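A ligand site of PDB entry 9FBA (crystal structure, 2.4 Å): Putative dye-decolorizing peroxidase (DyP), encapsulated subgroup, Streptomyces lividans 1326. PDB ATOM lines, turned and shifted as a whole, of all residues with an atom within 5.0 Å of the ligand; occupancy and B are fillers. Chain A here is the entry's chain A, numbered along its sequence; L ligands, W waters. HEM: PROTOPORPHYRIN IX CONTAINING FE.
The backbone NH (N) of Gly 153 is in hydrogen-bond range of an oxygen (O1A) of the ligand, 2.9 Å away. The backbone NH (N) of Thr 154 sits at hydrogen-bond distance from an oxygen (O1A) of the ligand (3.3 Å). The backbone NH (N) of Glu 155 is in hydrogen-bond range of an oxygen (O2A) of the ligand (3.3 Å). OG of Ser 230 lies within hydrogen-bond range of O1D of the ligand. An iron atom (FE) of the ligand is bound by a ring nitrogen (NE2) of His 225 (2.1 Å). O1A of the ligand is in salt-bridge range of NH1 of Arg 243 (2.9 Å).
The side-chain carboxylate (OD1) of Asp 212 lies within salt-bridge range of the guanidinium group (NE) of Arg 207 (3.0 Å). OH of Tyr 186 is in hydrogen-bond range of OE1 of Gln 184 (2.6 Å). OD1 of Asp 146 lies close to N of Leu 148 (3.1 Å). The backbone NH (N) of Phe 150 sits at hydrogen-bond distance from the side-chain carboxylate (OD1) of Asp 146 (3.3 Å). OD1 of Asp 152 lies within salt-bridge range of NH1 of Arg 243. O of Val 226 lies within hydrogen-bond range of OG of Ser 230, 3.4 Å away. OD1 of Asp 152 lies within hydrogen-bond range of ND2 of Asn 245. The backbone carbonyl oxygen (O) of Ile 289 sits at hydrogen-bond distance from the side-chain hydroxyl (OG) of Ser 293 (2.7 Å).
OD2 of Asp 146 touches CMB of the ligand (3.2 Å). Phe 150 touches the ligand (CB to CMA, 3.9 Å). Val 151 touches the ligand. Asp 152 touches the ligand (OD2 to CHB, 3.5 Å). Gln 184 touches the ligand (OE1 to CMC, 3.6 Å). CD2 of Tyr 186 touches CBB of the ligand, 3.6 Å away. His 188 touches the ligand. Arg 207 touches the ligand (CD to CAA, 3.4 Å). Thr 229 touches the ligand (OG1 to C2D, 3.6 Å). Asn 245 touches the ligand. Thr 258 touches the ligand. Phe 260 touches the ligand. Met 273 touches the ligand (CE to CMD, 3.7 Å). Leu 274 touches the ligand. Met 277 touches the ligand. Ile 289 touches the ligand. 22 residues have an atom within 4 Å of the ligand: Asp 146, Phe 150, Val 151, Asp 152, Gly 153, Thr 154, Glu 155, Gln 184, Tyr 186, His 188, Arg 207, His 225, Thr 229, Ser 230, Arg 243, Asn 245, Thr 258, Phe 260, Met 273, Leu 274, Met 277 and Ile 289.
Water W1 bridges OE1 of Glu 155 (2.7 Å) and O1D of the ligand (2.9 Å).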
ATOM      1  N   ASP A 146      14.226 -14.312 -24.446  1.00  0.00           N
ATOM      2  CA  ASP A 146      14.663 -13.649 -25.651  1.00  0.00           C
ATOM      3  C   ASP A 146      15.672 -12.620 -25.205  1.00  0.00           C
ATOM      4  O   ASP A 146      16.074 -12.609 -24.048  1.00  0.00           O
ATOM      5  CB  ASP A 146      13.493 -13.066 -26.441  1.00  0.00           C
ATOM      6  CG  ASP A 146      12.648 -12.061 -25.667  1.00  0.00           C
ATOM      7  OD1 ASP A 146      13.165 -11.530 -24.677  1.00  0.00           O
ATOM      8  OD2 ASP A 146      11.470 -11.893 -26.038  1.00  0.00           O
ATOM      9  N   LEU A 148      15.613  -9.573 -24.744  1.00  0.00           N
ATOM     10  CA  LEU A 148      15.193  -8.527 -23.822  1.00  0.00           C
ATOM     11  C   LEU A 148      15.057  -9.052 -22.393  1.00  0.00           C
ATOM     12  O   LEU A 148      14.787  -8.277 -21.487  1.00  0.00           O
ATOM     13  CB  LEU A 148      13.857  -7.995 -24.296  1.00  0.00           C
ATOM     14  CG  LEU A 148      13.885  -7.331 -25.666  1.00  0.00           C
ATOM     15  CD1 LEU A 148      12.507  -6.799 -25.903  1.00  0.00           C
ATOM     16  CD2 LEU A 148      14.910  -6.229 -25.741  1.00  0.00           C
ATOM     17  N   PHE A 150      12.846 -11.526 -21.345  1.00  0.00           N
ATOM     18  CA  PHE A 150      11.526 -12.060 -21.032  1.00  0.00           C
ATOM     19  C   PHE A 150      11.256 -13.429 -21.679  1.00  0.00           C
ATOM     20  O   PHE A 150      11.793 -13.750 -22.760  1.00  0.00           O
ATOM     21  CB  PHE A 150      10.408 -11.161 -21.520  1.00  0.00           C
ATOM     22  CG  PHE A 150      10.217  -9.959 -20.617  1.00  0.00           C
ATOM     23  CD1 PHE A 150      11.185  -8.992 -20.534  1.00  0.00           C
ATOM     24  CD2 PHE A 150       9.085  -9.813 -19.867  1.00  0.00           C
ATOM     25  CE1 PHE A 150      10.999  -7.872 -19.735  1.00  0.00           C
ATOM     26  CE2 PHE A 150       8.899  -8.692 -19.068  1.00  0.00           C
ATOM     27  CZ  PHE A 150       9.854  -7.744 -18.987  1.00  0.00           C
ATOM     28  N   VAL A 151      10.373 -14.189 -21.043  1.00  0.00           N
ATOM     29  CA  VAL A 151      10.048 -15.492 -21.584  1.00  0.00           C
ATOM     30  C   VAL A 151       9.188 -15.253 -22.814  1.00  0.00           C
ATOM     31  O   VAL A 151       8.269 -14.413 -22.746  1.00  0.00           O
ATOM     32  CB  VAL A 151       9.319 -16.353 -20.532  1.00  0.00           C
ATOM     33  CG1 VAL A 151       8.950 -17.725 -21.062  1.00  0.00           C
ATOM     34  CG2 VAL A 151      10.079 -16.472 -19.233  1.00  0.00           C
ATOM     35  N   ASP A 152       9.534 -15.984 -23.899  1.00  0.00           N
ATOM     36  CA  ASP A 152       9.066 -15.745 -25.260  1.00  0.00           C
ATOM     37  C   ASP A 152       8.492 -17.036 -25.860  1.00  0.00           C
ATOM     38  O   ASP A 152       9.227 -17.967 -26.243  1.00  0.00           O
ATOM     39  CB  ASP A 152      10.176 -15.171 -26.150  1.00  0.00           C
ATOM     40  CG  ASP A 152       9.772 -14.568 -27.499  1.00  0.00           C
ATOM     41  OD1 ASP A 152       8.812 -15.102 -28.123  1.00  0.00           O
ATOM     42  OD2 ASP A 152      10.470 -13.603 -27.974  1.00  0.00           O
ATOM     43  N   GLY A 153       7.168 -17.047 -25.965  1.00  0.00           N
ATOM     44  CA  GLY A 153       6.419 -18.148 -26.556  1.00  0.00           C
ATOM     45  C   GLY A 153       5.180 -18.581 -25.761  1.00  0.00           C
ATOM     46  O   GLY A 153       4.415 -19.422 -26.214  1.00  0.00           O
ATOM     47  N   THR A 154       4.988 -18.000 -24.566  1.00  0.00           N
ATOM     48  CA  THR A 154       4.139 -18.516 -23.501  1.00  0.00           C
ATOM     49  C   THR A 154       2.704 -18.695 -23.964  1.00  0.00           C
ATOM     50  O   THR A 154       2.132 -19.751 -23.726  1.00  0.00           O
ATOM     51  CB  THR A 154       4.224 -17.550 -22.321  1.00  0.00           C
ATOM     52  OG1 THR A 154       5.621 -17.386 -21.996  1.00  0.00           O
ATOM     53  CG2 THR A 154       3.443 -18.010 -21.101  1.00  0.00           C
ATOM     54  N   GLU A 155       2.144 -17.678 -24.655  1.00  0.00           N
ATOM     55  CA  GLU A 155       0.735 -17.634 -25.035  1.00  0.00           C
ATOM     56  C   GLU A 155       0.490 -18.165 -26.459  1.00  0.00           C
ATOM     57  O   GLU A 155      -0.576 -18.015 -27.025  1.00  0.00           O
ATOM     58  CB  GLU A 155       0.197 -16.221 -24.848  1.00  0.00           C
ATOM     59  CG  GLU A 155      -0.150 -15.927 -23.383  1.00  0.00           C
ATOM     60  CD  GLU A 155      -1.584 -16.316 -23.063  1.00  0.00           C
ATOM     61  OE1 GLU A 155      -2.564 -15.698 -23.600  1.00  0.00           O
ATOM     62  OE2 GLU A 155      -1.671 -17.278 -22.269  1.00  0.00           O
ATOM     63  N   GLN A 184      10.505 -11.218 -39.887  1.00  0.00           N
ATOM     64  CA  GLN A 184      11.135  -9.917 -39.704  1.00  0.00           C
ATOM     65  C   GLN A 184      12.381 -10.115 -38.837  1.00  0.00           C
ATOM     66  O   GLN A 184      12.303 -10.717 -37.766  1.00  0.00           O
ATOM     67  CB  GLN A 184      10.216  -8.986 -38.934  1.00  0.00           C
ATOM     68  CG  GLN A 184       9.017  -8.498 -39.722  1.00  0.00           C
ATOM     69  CD  GLN A 184       8.252  -7.463 -38.965  1.00  0.00           C
ATOM     70  OE1 GLN A 184       7.708  -7.782 -37.896  1.00  0.00           O
ATOM     71  NE2 GLN A 184       8.328  -6.220 -39.457  1.00  0.00           N
ATOM     72  N   TYR A 186      14.705  -8.391 -36.279  1.00  0.00           N
ATOM     73  CA  TYR A 186      14.729  -7.211 -35.414  1.00  0.00           C
ATOM     74  C   TYR A 186      16.069  -7.150 -34.706  1.00  0.00           C
ATOM     75  O   TYR A 186      16.635  -8.167 -34.309  1.00  0.00           O
ATOM     76  CB  TYR A 186      13.646  -7.216 -34.347  1.00  0.00           C
ATOM     77  CG  TYR A 186      12.234  -6.907 -34.810  1.00  0.00           C
ATOM     78  CD1 TYR A 186      11.781  -5.598 -34.917  1.00  0.00           C
ATOM     79  CD2 TYR A 186      11.342  -7.922 -35.116  1.00  0.00           C
ATOM     80  CE1 TYR A 186      10.492  -5.309 -35.300  1.00  0.00           C
ATOM     81  CE2 TYR A 186      10.046  -7.650 -35.532  1.00  0.00           C
ATOM     82  CZ  TYR A 186       9.606  -6.333 -35.606  1.00  0.00           C
ATOM     83  OH  TYR A 186       8.342  -6.032 -36.036  1.00  0.00           O
ATOM     84  N   HIS A 188      17.941  -5.019 -31.424  1.00  0.00           N
ATOM     85  CA  HIS A 188      17.554  -4.293 -30.224  1.00  0.00           C
ATOM     86  C   HIS A 188      18.666  -3.336 -29.815  1.00  0.00           C
ATOM     87  O   HIS A 188      19.837  -3.597 -30.097  1.00  0.00           O
ATOM     88  CB  HIS A 188      17.228  -5.277 -29.114  1.00  0.00           C
ATOM     89  CG  HIS A 188      16.185  -6.293 -29.403  1.00  0.00           C
ATOM     90  ND1 HIS A 188      14.851  -5.943 -29.457  1.00  0.00           N
ATOM     91  CD2 HIS A 188      16.238  -7.631 -29.694  1.00  0.00           C
ATOM     92  CE1 HIS A 188      14.131  -7.035 -29.708  1.00  0.00           C
ATOM     93  NE2 HIS A 188      14.951  -8.100 -29.830  1.00  0.00           N
ATOM     94  N   ILE A 205       6.247  -4.679 -21.946  1.00  0.00           N
ATOM     95  CA  ILE A 205       5.908  -5.978 -22.479  1.00  0.00           C
ATOM     96  C   ILE A 205       4.470  -6.333 -22.108  1.00  0.00           C
ATOM     97  O   ILE A 205       3.731  -6.795 -22.969  1.00  0.00           O
ATOM     98  CB  ILE A 205       6.909  -7.029 -21.964  1.00  0.00           C
ATOM     99  CG1 ILE A 205       8.289  -6.756 -22.469  1.00  0.00           C
ATOM    100  CG2 ILE A 205       6.457  -8.458 -22.307  1.00  0.00           C
ATOM    101  CD1 ILE A 205       8.545  -7.189 -23.902  1.00  0.00           C
ATOM    102  N   ARG A 207       3.921  -8.348 -19.215  1.00  0.00           N
ATOM    103  CA  ARG A 207       4.021  -9.464 -18.286  1.00  0.00           C
ATOM    104  C   ARG A 207       5.126  -9.219 -17.265  1.00  0.00           C
ATOM    105  O   ARG A 207       5.964  -8.334 -17.437  1.00  0.00           O
ATOM    106  CB  ARG A 207       4.330 -10.766 -19.032  1.00  0.00           C
ATOM    107  CG  ARG A 207       3.551 -11.019 -20.307  1.00  0.00           C
ATOM    108  CD  ARG A 207       3.913 -12.367 -20.945  1.00  0.00           C
ATOM    109  NE  ARG A 207       3.387 -13.521 -20.206  1.00  0.00           N
ATOM    110  CZ  ARG A 207       2.125 -13.987 -20.297  1.00  0.00           C
ATOM    111  NH1 ARG A 207       1.193 -13.353 -21.029  1.00  0.00           N
ATOM    112  NH2 ARG A 207       1.806 -15.091 -19.646  1.00  0.00           N
ATOM    113  N   ASP A 212       6.809 -14.436 -15.379  1.00  0.00           N
ATOM    114  CA  ASP A 212       6.115 -14.552 -16.646  1.00  0.00           C
ATOM    115  C   ASP A 212       4.601 -14.685 -16.472  1.00  0.00           C
ATOM    116  O   ASP A 212       3.949 -15.315 -17.304  1.00  0.00           O
ATOM    117  CB  ASP A 212       6.611 -15.734 -17.450  1.00  0.00           C
ATOM    118  CG  ASP A 212       6.190 -15.805 -18.905  1.00  0.00           C
ATOM    119  OD1 ASP A 212       6.051 -14.685 -19.557  1.00  0.00           O
ATOM    120  OD2 ASP A 212       6.136 -17.015 -19.371  1.00  0.00           O
ATOM    121  N   GLU A 214       0.928 -12.698 -16.612  1.00  0.00           N
ATOM    122  CA  GLU A 214       0.282 -11.530 -17.219  1.00  0.00           C
ATOM    123  C   GLU A 214       0.105 -10.416 -16.186  1.00  0.00           C
ATOM    124  O   GLU A 214      -0.235 -10.666 -15.042  1.00  0.00           O
ATOM    125  CB  GLU A 214      -1.049 -12.001 -17.828  1.00  0.00           C
ATOM    126  CG  GLU A 214      -1.584 -11.105 -18.944  1.00  0.00           C
ATOM    127  CD  GLU A 214      -2.457 -11.739 -20.013  1.00  0.00           C
ATOM    128  OE1 GLU A 214      -2.318 -12.903 -20.477  1.00  0.00           O
ATOM    129  OE2 GLU A 214      -3.289 -10.935 -20.460  1.00  0.00           O
ATOM    130  N   HIS A 225       3.130  -4.408 -25.390  1.00  0.00           N
ATOM    131  CA  HIS A 225       3.208  -5.308 -26.523  1.00  0.00           C
ATOM    132  C   HIS A 225       2.071  -6.324 -26.472  1.00  0.00           C
ATOM    133  O   HIS A 225       1.463  -6.610 -27.509  1.00  0.00           O
ATOM    134  CB  HIS A 225       4.544  -6.068 -26.523  1.00  0.00           C
ATOM    135  CG  HIS A 225       4.716  -7.064 -27.634  1.00  0.00           C
ATOM    136  ND1 HIS A 225       4.626  -6.711 -28.943  1.00  0.00           N
ATOM    137  CD2 HIS A 225       5.054  -8.394 -27.658  1.00  0.00           C
ATOM    138  CE1 HIS A 225       4.866  -7.778 -29.691  1.00  0.00           C
ATOM    139  NE2 HIS A 225       5.074  -8.822 -28.945  1.00  0.00           N
ATOM    140  N   VAL A 226       1.791  -6.870 -25.279  1.00  0.00           N
ATOM    141  CA  VAL A 226       0.766  -7.877 -25.109  1.00  0.00           C
ATOM    142  C   VAL A 226      -0.621  -7.268 -25.335  1.00  0.00           C
ATOM    143  O   VAL A 226      -1.531  -7.949 -25.784  1.00  0.00           O
ATOM    144  CB  VAL A 226       0.864  -8.598 -23.752  1.00  0.00           C
ATOM    145  CG1 VAL A 226      -0.490  -9.058 -23.209  1.00  0.00           C
ATOM    146  CG2 VAL A 226       1.860  -9.770 -23.819  1.00  0.00           C
ATOM    147  N   THR A 229      -1.140  -6.796 -29.238  1.00  0.00           N
ATOM    148  CA  THR A 229      -1.122  -8.008 -30.046  1.00  0.00           C
ATOM    149  C   THR A 229      -2.209  -9.011 -29.602  1.00  0.00           C
ATOM    150  O   THR A 229      -2.270 -10.136 -30.096  1.00  0.00           O
ATOM    151  CB  THR A 229       0.282  -8.627 -30.021  1.00  0.00           C
ATOM    152  OG1 THR A 229       0.663  -8.891 -28.674  1.00  0.00           O
ATOM    153  CG2 THR A 229       1.357  -7.728 -30.602  1.00  0.00           C
ATOM    154  N   SER A 230      -3.076  -8.634 -28.651  1.00  0.00           N
ATOM    155  CA  SER A 230      -4.321  -9.347 -28.404  1.00  0.00           C
ATOM    156  C   SER A 230      -5.421  -8.754 -29.295  1.00  0.00           C
ATOM    157  O   SER A 230      -5.814  -7.614 -29.084  1.00  0.00           O
ATOM    158  CB  SER A 230      -4.768  -9.288 -26.953  1.00  0.00           C
ATOM    159  OG  SER A 230      -4.034 -10.195 -26.151  1.00  0.00           O
ATOM    160  N   ILE A 241      -1.869 -16.324 -33.731  1.00  0.00           N
ATOM    161  CA  ILE A 241      -0.822 -16.850 -34.588  1.00  0.00           C
ATOM    162  C   ILE A 241       0.155 -17.730 -33.808  1.00  0.00           C
ATOM    163  O   ILE A 241       0.214 -17.728 -32.573  1.00  0.00           O
ATOM    164  CB  ILE A 241      -0.036 -15.724 -35.277  1.00  0.00           C
ATOM    165  CG1 ILE A 241       0.851 -14.996 -34.314  1.00  0.00           C
ATOM    166  CG2 ILE A 241      -0.968 -14.759 -35.987  1.00  0.00           C
ATOM    167  CD1 ILE A 241       1.758 -13.962 -34.947  1.00  0.00           C
ATOM    168  N   ARG A 243       4.149 -18.318 -33.205  1.00  0.00           N
ATOM    169  CA  ARG A 243       5.448 -17.681 -33.263  1.00  0.00           C
ATOM    170  C   ARG A 243       6.523 -18.673 -32.826  1.00  0.00           C
ATOM    171  O   ARG A 243       6.248 -19.566 -32.029  1.00  0.00           O
ATOM    172  CB  ARG A 243       5.541 -16.516 -32.287  1.00  0.00           C
ATOM    173  CG  ARG A 243       4.627 -15.367 -32.684  1.00  0.00           C
ATOM    174  CD  ARG A 243       4.429 -14.340 -31.586  1.00  0.00           C
ATOM    175  NE  ARG A 243       3.608 -14.945 -30.540  1.00  0.00           N
ATOM    176  CZ  ARG A 243       4.008 -15.066 -29.287  1.00  0.00           C
ATOM    177  NH1 ARG A 243       5.204 -14.656 -28.904  1.00  0.00           N
ATOM    178  NH2 ARG A 243       3.190 -15.608 -28.390  1.00  0.00           N
ATOM    179  N   ASN A 245       9.995 -17.199 -32.173  1.00  0.00           N
ATOM    180  CA  ASN A 245      11.050 -16.211 -32.126  1.00  0.00           C
ATOM    181  C   ASN A 245      12.319 -16.881 -31.627  1.00  0.00           C
ATOM    182  O   ASN A 245      12.276 -17.663 -30.658  1.00  0.00           O
ATOM    183  CB  ASN A 245      10.721 -15.036 -31.205  1.00  0.00           C
ATOM    184  CG  ASN A 245       9.467 -14.310 -31.629  1.00  0.00           C
ATOM    185  OD1 ASN A 245       8.967 -14.564 -32.728  1.00  0.00           O
ATOM    186  ND2 ASN A 245       8.950 -13.421 -30.788  1.00  0.00           N
ATOM    187  N   THR A 258      16.274 -10.359 -32.203  1.00  0.00           N
ATOM    188  CA  THR A 258      15.240 -11.376 -32.146  1.00  0.00           C
ATOM    189  C   THR A 258      14.732 -11.549 -33.578  1.00  0.00           C
ATOM    190  O   THR A 258      14.369 -10.571 -34.219  1.00  0.00           O
ATOM    191  CB  THR A 258      14.190 -10.945 -31.110  1.00  0.00           C
ATOM    192  OG1 THR A 258      14.709 -11.261 -29.794  1.00  0.00           O
ATOM    193  CG2 THR A 258      12.870 -11.622 -31.400  1.00  0.00           C
ATOM    194  N   PHE A 260      11.923 -12.817 -35.903  1.00  0.00           N
ATOM    195  CA  PHE A 260      10.509 -13.019 -35.685  1.00  0.00           C
ATOM    196  C   PHE A 260       9.965 -13.855 -36.822  1.00  0.00           C
ATOM    197  O   PHE A 260      10.199 -13.549 -37.990  1.00  0.00           O
ATOM    198  CB  PHE A 260       9.734 -11.708 -35.670  1.00  0.00           C
ATOM    199  CG  PHE A 260       8.242 -11.932 -35.728  1.00  0.00           C
ATOM    200  CD1 PHE A 260       7.529 -12.315 -34.607  1.00  0.00           C
ATOM    201  CD2 PHE A 260       7.556 -11.790 -36.924  1.00  0.00           C
ATOM    202  CE1 PHE A 260       6.165 -12.539 -34.676  1.00  0.00           C
ATOM    203  CE2 PHE A 260       6.186 -12.006 -36.983  1.00  0.00           C
ATOM    204  CZ  PHE A 260       5.496 -12.366 -35.868  1.00  0.00           C
ATOM    205  N   THR A 270      -1.945 -11.760 -38.953  1.00  0.00           N
ATOM    206  CA  THR A 270      -0.585 -11.314 -38.695  1.00  0.00           C
ATOM    207  C   THR A 270      -0.492  -9.815 -39.023  1.00  0.00           C
ATOM    208  O   THR A 270       0.089  -9.024 -38.288  1.00  0.00           O
ATOM    209  CB  THR A 270       0.405 -12.152 -39.511  1.00  0.00           C
ATOM    210  OG1 THR A 270       0.505 -13.580 -39.382  1.00  0.00           O
ATOM    211  CG2 THR A 270       1.811 -11.788 -39.127  1.00  0.00           C
ATOM    212  N   MET A 273      -2.030  -7.355 -36.444  1.00  0.00           N
ATOM    213  CA  MET A 273      -1.197  -7.159 -35.295  1.00  0.00           C
ATOM    214  C   MET A 273      -0.109  -6.149 -35.637  1.00  0.00           C
ATOM    215  O   MET A 273       0.255  -5.323 -34.823  1.00  0.00           O
ATOM    216  CB  MET A 273      -0.609  -8.503 -34.865  1.00  0.00           C
ATOM    217  CG  MET A 273      -1.618  -9.459 -34.285  1.00  0.00           C
ATOM    218  SD  MET A 273      -0.913 -11.133 -34.223  1.00  0.00           S
ATOM    219  CE  MET A 273      -2.191 -12.013 -33.329  1.00  0.00           C
ATOM    220  N   LEU A 274       0.395  -6.190 -36.876  1.00  0.00           N
ATOM    221  CA  LEU A 274       1.487  -5.340 -37.274  1.00  0.00           C
ATOM    222  C   LEU A 274       1.042  -3.880 -37.364  1.00  0.00           C
ATOM    223  O   LEU A 274       1.772  -2.990 -36.936  1.00  0.00           O
ATOM    224  CB  LEU A 274       2.059  -5.837 -38.599  1.00  0.00           C
ATOM    225  CG  LEU A 274       3.044  -7.019 -38.507  1.00  0.00           C
ATOM    226  CD1 LEU A 274       3.431  -7.648 -39.815  1.00  0.00           C
ATOM    227  CD2 LEU A 274       4.351  -6.559 -37.862  1.00  0.00           C
ATOM    228  N   MET A 277       0.828  -2.460 -34.108  1.00  0.00           N
ATOM    229  CA  MET A 277       2.135  -2.208 -33.541  1.00  0.00           C
ATOM    230  C   MET A 277       2.774  -0.951 -34.127  1.00  0.00           C
ATOM    231  O   MET A 277       3.302  -0.154 -33.369  1.00  0.00           O
ATOM    232  CB  MET A 277       3.044  -3.424 -33.765  1.00  0.00           C
ATOM    233  CG  MET A 277       2.768  -4.571 -32.825  1.00  0.00           C
ATOM    234  SD  MET A 277       3.709  -6.023 -33.356  1.00  0.00           S
ATOM    235  CE  MET A 277       5.368  -5.476 -32.946  1.00  0.00           C
ATOM    236  N   ILE A 289       7.494  -1.723 -27.614  1.00  0.00           N
ATOM    237  CA  ILE A 289       8.606  -2.614 -27.836  1.00  0.00           C
ATOM    238  C   ILE A 289       9.456  -2.125 -29.013  1.00  0.00           C
ATOM    239  O   ILE A 289      10.630  -2.477 -29.095  1.00  0.00           O
ATOM    240  CB  ILE A 289       8.107  -4.062 -28.045  1.00  0.00           C
ATOM    241  CG1 ILE A 289       9.220  -5.047 -27.652  1.00  0.00           C
ATOM    242  CG2 ILE A 289       7.608  -4.297 -29.467  1.00  0.00           C
ATOM    243  CD1 ILE A 289       8.821  -6.511 -27.663  1.00  0.00           C
ATOM    244  N   SER A 293      13.457  -1.807 -30.616  1.00  0.00           N
ATOM    245  CA  SER A 293      13.621  -2.847 -31.608  1.00  0.00           C
ATOM    246  C   SER A 293      13.438  -2.218 -32.982  1.00  0.00           C
ATOM    247  O   SER A 293      12.465  -1.524 -33.201  1.00  0.00           O
ATOM    248  CB  SER A 293      12.653  -3.980 -31.373  1.00  0.00           C
ATOM    249  OG  SER A 293      12.431  -4.224 -29.998  1.00  0.00           O
HETATM  250  CHA HEM L   1       3.746 -12.007 -27.045  1.00  0.00           C
HETATM  251  CHB HEM L   1       8.368 -10.843 -27.448  1.00  0.00           C
HETATM  252  CHC HEM L   1       7.601  -9.206 -31.987  1.00  0.00           C
HETATM  253  CHD HEM L   1       3.156 -11.164 -31.634  1.00  0.00           C
HETATM  254  C1A HEM L   1       5.071 -11.795 -26.780  1.00  0.00           C
HETATM  255  C2A HEM L   1       5.618 -11.971 -25.475  1.00  0.00           C
HETATM  256  C3A HEM L   1       6.944 -11.653 -25.612  1.00  0.00           C
HETATM  257  C4A HEM L   1       7.192 -11.256 -26.947  1.00  0.00           C
HETATM  258  CMA HEM L   1       7.904 -11.729 -24.472  1.00  0.00           C
HETATM  259  CAA HEM L   1       4.941 -12.440 -24.159  1.00  0.00           C
HETATM  260  CBA HEM L   1       5.301 -13.929 -23.952  1.00  0.00           C
HETATM  261  CGA HEM L   1       4.493 -14.609 -25.053  1.00  0.00           C
HETATM  262  O1A HEM L   1       5.062 -15.093 -26.075  1.00  0.00           O
HETATM  263  O2A HEM L   1       3.214 -14.575 -24.958  1.00  0.00           O
HETATM  264  C1B HEM L   1       8.520 -10.291 -28.722  1.00  0.00           C
HETATM  265  C2B HEM L   1       9.733  -9.750 -29.111  1.00  0.00           C
HETATM  266  C3B HEM L   1       9.593  -9.284 -30.352  1.00  0.00           C
HETATM  267  C4B HEM L   1       8.191  -9.545 -30.752  1.00  0.00           C
HETATM  268  CMB HEM L   1      11.019  -9.693 -28.341  1.00  0.00           C
HETATM  269  CAB HEM L   1      10.677  -8.518 -30.967  1.00  0.00           C
HETATM  270  CBB HEM L   1      10.401  -7.415 -31.640  1.00  0.00           C
HETATM  271  C1C HEM L   1       6.311  -9.576 -32.353  1.00  0.00           C
HETATM  272  C2C HEM L   1       5.627  -9.366 -33.577  1.00  0.00           C
HETATM  273  C3C HEM L   1       4.363  -9.924 -33.439  1.00  0.00           C
HETATM  274  C4C HEM L   1       4.291 -10.488 -32.123  1.00  0.00           C
HETATM  275  CMC HEM L   1       6.150  -8.669 -34.788  1.00  0.00           C
HETATM  276  CAC HEM L   1       3.196 -10.027 -34.354  1.00  0.00           C
HETATM  277  CBC HEM L   1       3.138  -9.515 -35.550  1.00  0.00           C
HETATM  278  C1D HEM L   1       2.947 -11.553 -30.344  1.00  0.00           C
HETATM  279  C2D HEM L   1       1.688 -12.138 -29.892  1.00  0.00           C
HETATM  280  C3D HEM L   1       1.801 -12.329 -28.554  1.00  0.00           C
HETATM  281  C4D HEM L   1       3.197 -11.886 -28.301  1.00  0.00           C
HETATM  282  CMD HEM L   1       0.490 -12.403 -30.777  1.00  0.00           C
HETATM  283  CAD HEM L   1       0.806 -12.949 -27.526  1.00  0.00           C
HETATM  284  CBD HEM L   1      -0.545 -12.210 -27.104  1.00  0.00           C
HETATM  285  CGD HEM L   1      -1.310 -12.762 -25.824  1.00  0.00           C
HETATM  286  O1D HEM L   1      -2.565 -13.127 -25.810  1.00  0.00           O
HETATM  287  O2D HEM L   1      -0.654 -12.821 -24.711  1.00  0.00           O
HETATM  288  NA  HEM L   1       6.044 -11.306 -27.675  1.00  0.00           N
HETATM  289  NB  HEM L   1       7.648 -10.171 -29.714  1.00  0.00           N
HETATM  290  NC  HEM L   1       5.481 -10.264 -31.524  1.00  0.00           N
HETATM  291  ND  HEM L   1       3.845 -11.411 -29.399  1.00  0.00           N
HETATM  292 FE   HEM L   1       5.672 -10.770 -29.588  1.00  0.00          FE
HETATM  293  O   HOH W   1      -4.512 -13.764 -23.756  1.00  0.00           O
